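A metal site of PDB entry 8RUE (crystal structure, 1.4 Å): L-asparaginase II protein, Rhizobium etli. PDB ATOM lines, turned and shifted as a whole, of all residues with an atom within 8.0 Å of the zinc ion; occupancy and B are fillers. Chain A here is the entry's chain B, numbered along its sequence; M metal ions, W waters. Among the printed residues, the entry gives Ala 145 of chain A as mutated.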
ATOM      1  N   ARG A  53       0.492  18.235 -30.271  1.00  0.00           N
ATOM      2  CA  ARG A  53       1.640  17.612 -29.618  1.00  0.00           C
ATOM      3  C   ARG A  53       1.847  18.313 -28.269  1.00  0.00           C
ATOM      4  O   ARG A  53       0.861  18.601 -27.558  1.00  0.00           O
ATOM      5  CB  ARG A  53       2.869  17.568 -30.538  1.00  0.00           C
ATOM      6  CG  ARG A  53       2.583  16.938 -31.894  1.00  0.00           C
ATOM      7  CD  ARG A  53       2.317  15.409 -31.842  1.00  0.00           C
ATOM      8  NE  ARG A  53       3.472  14.668 -31.369  1.00  0.00           N
ATOM      9  CZ  ARG A  53       4.567  14.506 -32.100  1.00  0.00           C
ATOM     10  NH1 ARG A  53       4.639  14.944 -33.353  1.00  0.00           N
ATOM     11  NH2 ARG A  53       5.620  13.893 -31.553  1.00  0.00           N
ATOM     12  N   SER A  54       3.090  18.653 -27.916  1.00  0.00           N
ATOM     13  CA  SER A  54       3.348  19.254 -26.604  1.00  0.00           C
ATOM     14  C   SER A  54       2.727  20.616 -26.430  1.00  0.00           C
ATOM     15  O   SER A  54       2.664  21.092 -25.296  1.00  0.00           O
ATOM     16  CB  SER A  54       4.855  19.380 -26.339  1.00  0.00           C
ATOM     17  OG  SER A  54       5.416  18.099 -26.134  1.00  0.00           O
ATOM     18  N   LYS A  57       0.075  20.739 -23.852  1.00  0.00           N
ATOM     19  CA  LYS A  57       0.366  20.427 -22.450  1.00  0.00           C
ATOM     20  C   LYS A  57      -0.328  21.337 -21.460  1.00  0.00           C
ATOM     21  O   LYS A  57      -0.737  20.818 -20.411  1.00  0.00           O
ATOM     22  CB  LYS A  57       1.869  20.312 -22.189  1.00  0.00           C
ATOM     23  CG  LYS A  57       2.412  18.999 -22.673  1.00  0.00           C
ATOM     24  CD  LYS A  57       3.950  18.999 -22.710  1.00  0.00           C
ATOM     25  CE  LYS A  57       4.460  17.622 -23.078  1.00  0.00           C
ATOM     26  NZ  LYS A  57       5.955  17.628 -23.343  1.00  0.00           N
ATOM     27  N   GLN A  60      -3.667  19.760 -20.894  1.00  0.00           N
ATOM     28  CA  GLN A  60      -3.543  18.558 -20.085  1.00  0.00           C
ATOM     29  C   GLN A  60      -3.257  18.891 -18.623  1.00  0.00           C
ATOM     30  O   GLN A  60      -3.773  18.217 -17.723  1.00  0.00           O
ATOM     31  CB  GLN A  60      -2.447  17.666 -20.676  1.00  0.00           C
ATOM     32  CG  GLN A  60      -2.862  17.074 -22.044  1.00  0.00           C
ATOM     33  CD  GLN A  60      -1.712  16.576 -22.868  1.00  0.00           C
ATOM     34  OE1 GLN A  60      -0.785  17.339 -23.194  1.00  0.00           O
ATOM     35  NE2 GLN A  60      -1.748  15.279 -23.188  1.00  0.00           N
ATOM     36  N   ALA A  85       5.817  21.204 -19.543  1.00  0.00           N
ATOM     37  CA  ALA A  85       7.099  21.300 -20.231  1.00  0.00           C
ATOM     38  C   ALA A  85       7.331  20.283 -21.346  1.00  0.00           C
ATOM     39  O   ALA A  85       6.798  19.172 -21.320  1.00  0.00           O
ATOM     40  CB  ALA A  85       8.189  21.010 -19.204  1.00  0.00           C
ATOM     41  N   SER A  86       8.238  20.660 -22.275  1.00  0.00           N
ATOM     42  CA  SER A  86       9.051  19.734 -23.110  1.00  0.00           C
ATOM     43  C   SER A  86      10.508  20.003 -22.714  1.00  0.00           C
ATOM     44  O   SER A  86      11.248  20.710 -23.415  1.00  0.00           O
ATOM     45  CB  SER A  86       8.906  19.952 -24.588  1.00  0.00           C
ATOM     46  OG  SER A  86       7.566  19.766 -24.985  1.00  0.00           O
ATOM     47  N   CYS A 113       5.792   6.407 -19.562  1.00  0.00           N
ATOM     48  CA  CYS A 113       6.540   7.037 -20.643  1.00  0.00           C
ATOM     49  C   CYS A 113       7.961   6.504 -20.622  1.00  0.00           C
ATOM     50  O   CYS A 113       8.407   5.952 -19.614  1.00  0.00           O
ATOM     51  CB  CYS A 113       6.541   8.575 -20.476  1.00  0.00           C
ATOM     52  SG  CYS A 113       7.194   9.164 -18.847  1.00  0.00           S
ATOM     53  N   SER A 139      12.184  11.600 -19.597  1.00  0.00           N
ATOM     54  CA  SER A 139      11.346  12.003 -20.714  1.00  0.00           C
ATOM     55  C   SER A 139      11.043  13.486 -20.639  1.00  0.00           C
ATOM     56  O   SER A 139      10.775  14.032 -19.558  1.00  0.00           O
ATOM     57  CB  SER A 139      10.013  11.252 -20.601  1.00  0.00           C
ATOM     58  OG  SER A 139       9.056  11.757 -21.515  1.00  0.00           O
ATOM     59  N   ASN A 140      11.020  14.144 -21.803  1.00  0.00           N
ATOM     60  CA  ASN A 140      10.618  15.541 -21.871  1.00  0.00           C
ATOM     61  C   ASN A 140       9.205  15.727 -21.368  1.00  0.00           C
ATOM     62  O   ASN A 140       8.852  16.848 -21.002  1.00  0.00           O
ATOM     63  CB  ASN A 140      10.744  16.108 -23.298  1.00  0.00           C
ATOM     64  CG  ASN A 140       9.577  15.742 -24.209  1.00  0.00           C
ATOM     65  OD1 ASN A 140       8.682  16.523 -24.441  1.00  0.00           O
ATOM     66  ND2 ASN A 140       9.628  14.546 -24.767  1.00  0.00           N
ATOM     67  N   CYS A 141       8.407  14.655 -21.343  1.00  0.00           N
ATOM     68  CA  CYS A 141       7.045  14.668 -20.845  1.00  0.00           C
ATOM     69  C   CYS A 141       6.928  14.120 -19.449  1.00  0.00           C
ATOM     70  O   CYS A 141       5.815  13.799 -19.011  1.00  0.00           O
ATOM     71  CB  CYS A 141       6.174  13.791 -21.739  1.00  0.00           C
ATOM     72  SG  CYS A 141       5.997  14.406 -23.478  1.00  0.00           S
ATOM     73  N   SER A 142       8.041  14.026 -18.704  1.00  0.00           N
ATOM     74  CA  SER A 142       7.989  13.372 -17.379  1.00  0.00           C
ATOM     75  C   SER A 142       7.092  14.108 -16.393  1.00  0.00           C
ATOM     76  O   SER A 142       6.458  13.462 -15.552  1.00  0.00           O
ATOM     77  CB  SER A 142       9.394  13.247 -16.798  1.00  0.00           C
ATOM     78  OG  SER A 142       9.960  14.539 -16.553  1.00  0.00           O
ATOM     79  N   LYS A 144       4.352  15.918 -17.053  1.00  0.00           N
ATOM     80  CA  LYS A 144       2.979  15.564 -17.407  1.00  0.00           C
ATOM     81  C   LYS A 144       2.652  14.140 -16.938  1.00  0.00           C
ATOM     82  O   LYS A 144       1.571  13.895 -16.379  1.00  0.00           O
ATOM     83  CB  LYS A 144       2.818  15.673 -18.914  1.00  0.00           C
ATOM     84  CG  LYS A 144       1.470  15.158 -19.441  1.00  0.00           C
ATOM     85  CD  LYS A 144       1.357  15.317 -20.963  1.00  0.00           C
ATOM     86  CE  LYS A 144       2.549  14.649 -21.704  1.00  0.00           C
ATOM     87  NZ  LYS A 144       2.343  14.535 -23.178  1.00  0.00           N
ATOM     88  N   ALA A 145       3.582  13.197 -17.135  1.00  0.00           N
ATOM     89  CA  ALA A 145       3.363  11.825 -16.685  1.00  0.00           C
ATOM     90  C   ALA A 145       3.104  11.756 -15.195  1.00  0.00           C
ATOM     91  O   ALA A 145       2.159  11.087 -14.746  1.00  0.00           O
ATOM     92  CB  ALA A 145       4.568  10.957 -17.046  1.00  0.00           C
ATOM     93  N   THR A 192      -1.400   8.843 -30.737  1.00  0.00           N
ATOM     94  CA  THR A 192      -0.568   8.516 -29.581  1.00  0.00           C
ATOM     95  C   THR A 192       0.753   9.245 -29.722  1.00  0.00           C
ATOM     96  O   THR A 192       1.359   9.230 -30.794  1.00  0.00           O
ATOM     97  CB  THR A 192      -0.344   6.992 -29.526  1.00  0.00           C
ATOM     98  OG1 THR A 192      -1.617   6.345 -29.372  1.00  0.00           O
ATOM     99  CG2 THR A 192       0.586   6.605 -28.364  1.00  0.00           C
ATOM    100  N   ASP A 193       1.215   9.875 -28.637  1.00  0.00           N
ATOM    101  CA  ASP A 193       2.402  10.710 -28.617  1.00  0.00           C
ATOM    102  C   ASP A 193       3.672   9.863 -28.408  1.00  0.00           C
ATOM    103  O   ASP A 193       3.611   8.666 -28.117  1.00  0.00           O
ATOM    104  CB  ASP A 193       2.250  11.782 -27.536  1.00  0.00           C
ATOM    105  CG  ASP A 193       2.708  13.140 -28.009  1.00  0.00           C
ATOM    106  OD1 ASP A 193       3.586  13.178 -28.895  1.00  0.00           O
ATOM    107  OD2 ASP A 193       2.164  14.173 -27.517  1.00  0.00           O
ATOM    108  N   GLY A 194       4.838  10.520 -28.516  1.00  0.00           N
ATOM    109  CA  GLY A 194       6.097   9.826 -28.246  1.00  0.00           C
ATOM    110  C   GLY A 194       6.207   9.262 -26.844  1.00  0.00           C
ATOM    111  O   GLY A 194       6.914   8.261 -26.621  1.00  0.00           O
ATOM    112  N   CYS A 195       5.520   9.879 -25.876  1.00  0.00           N
ATOM    113  CA  CYS A 195       5.529   9.444 -24.494  1.00  0.00           C
ATOM    114  C   CYS A 195       4.468   8.373 -24.211  1.00  0.00           C
ATOM    115  O   CYS A 195       4.350   7.927 -23.066  1.00  0.00           O
ATOM    116  CB  CYS A 195       5.286  10.655 -23.595  1.00  0.00           C
ATOM    117  SG  CYS A 195       3.625  11.367 -23.865  1.00  0.00           S
ATOM    118  N   ASN A 196       3.677   7.983 -25.221  1.00  0.00           N
ATOM    119  CA  ASN A 196       2.669   6.905 -25.184  1.00  0.00           C
ATOM    120  C   ASN A 196       1.335   7.350 -24.582  1.00  0.00           C
ATOM    121  O   ASN A 196       0.479   6.497 -24.294  1.00  0.00           O
ATOM    122  CB  ASN A 196       3.174   5.601 -24.543  1.00  0.00           C
ATOM    123  CG  ASN A 196       2.538   4.367 -25.166  1.00  0.00           C
ATOM    124  OD1 ASN A 196       2.232   4.344 -26.352  1.00  0.00           O
ATOM    125  ND2 ASN A 196       2.344   3.332 -24.354  1.00  0.00           N
ATOM    126  N   LEU A 197       1.098   8.665 -24.432  1.00  0.00           N
ATOM    127  CA  LEU A 197      -0.213   9.185 -24.040  1.00  0.00           C
ATOM    128  C   LEU A 197      -1.040   9.558 -25.260  1.00  0.00           C
ATOM    129  O   LEU A 197      -0.476   9.881 -26.314  1.00  0.00           O
ATOM    130  CB  LEU A 197      -0.025  10.471 -23.212  1.00  0.00           C
ATOM    131  CG  LEU A 197       0.359  10.269 -21.758  1.00  0.00           C
ATOM    132  CD1 LEU A 197       0.790  11.595 -21.180  1.00  0.00           C
ATOM    133  CD2 LEU A 197      -0.830   9.756 -20.992  1.00  0.00           C
ATOM    134  N   PRO A 198      -2.373   9.599 -25.137  1.00  0.00           N
ATOM    135  CA  PRO A 198      -3.187  10.161 -26.229  1.00  0.00           C
ATOM    136  C   PRO A 198      -2.798  11.612 -26.463  1.00  0.00           C
ATOM    137  O   PRO A 198      -2.492  12.354 -25.530  1.00  0.00           O
ATOM    138  CB  PRO A 198      -4.628  10.070 -25.703  1.00  0.00           C
ATOM    139  CG  PRO A 198      -4.559   9.017 -24.616  1.00  0.00           C
ATOM    140  CD  PRO A 198      -3.207   9.218 -23.980  1.00  0.00           C
ATOM    141  N   THR A 199      -2.870  12.033 -27.720  1.00  0.00           N
ATOM    142  CA  THR A 199      -2.493  13.408 -28.096  1.00  0.00           C
ATOM    143  C   THR A 199      -3.487  13.935 -29.129  1.00  0.00           C
ATOM    144  O   THR A 199      -3.895  13.188 -30.030  1.00  0.00           O
ATOM    145  CB  THR A 199      -1.026  13.445 -28.596  1.00  0.00           C
ATOM    146  OG1 THR A 199      -0.576  14.796 -28.676  1.00  0.00           O
ATOM    147  CG2 THR A 199      -0.855  12.701 -29.946  1.00  0.00           C
HETATM  148 ZN    ZN M   1       3.954  13.618 -24.143  1.00  0.00          ZN
HETATM  149  O   HOH W   1       3.761  15.175 -25.824  1.00  0.00           O
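SG of Cys 141 lies close to NZ of Lys 57, at 3.2 Å.
The side-chain amide oxygen (OD1) of Asn 140 sits close to the side-chain sulfur (SG) of Cys 141, 3.6 Å away.
The backbone NH (N) of Cys 141 lies close to the side-chain hydroxyl (OG) of Ser 139, 3.0 Å away.
The side-chain sulfur (SG) of Cys 195 lies close to the backbone NH (N) of Leu 197 (3.7 Å).
OD2 of Asp 193 is in hydrogen-bond range of OG1 of Thr 199, 3.0 Å away.
OD1 of Asp 193 lies within salt-bridge range of NE of Arg 53.
Merely in contact with the zinc ion: Asp 193.
Within 4 Å of the zinc ion: Cys 141, Lys 144, Asp 193 and Cys 195.
Along chain A the residues within 4 Å of the zinc ion span positions 141 to 195.
The nearest printed residue that does not touch the zinc ion is Lys 57 (4.2 Å).
NZ of Lys 144 is bound to the zinc ion, at 2.1 Å.
The zinc ion is bound by SG of Cys 141 (2.3 Å).
SG of Cys 195 binds the zinc ion.
Water W1 binds the zinc ion, at 2.3 Å.
Water W1 bridges OD2 of Asp 193 and OG of Ser 54.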
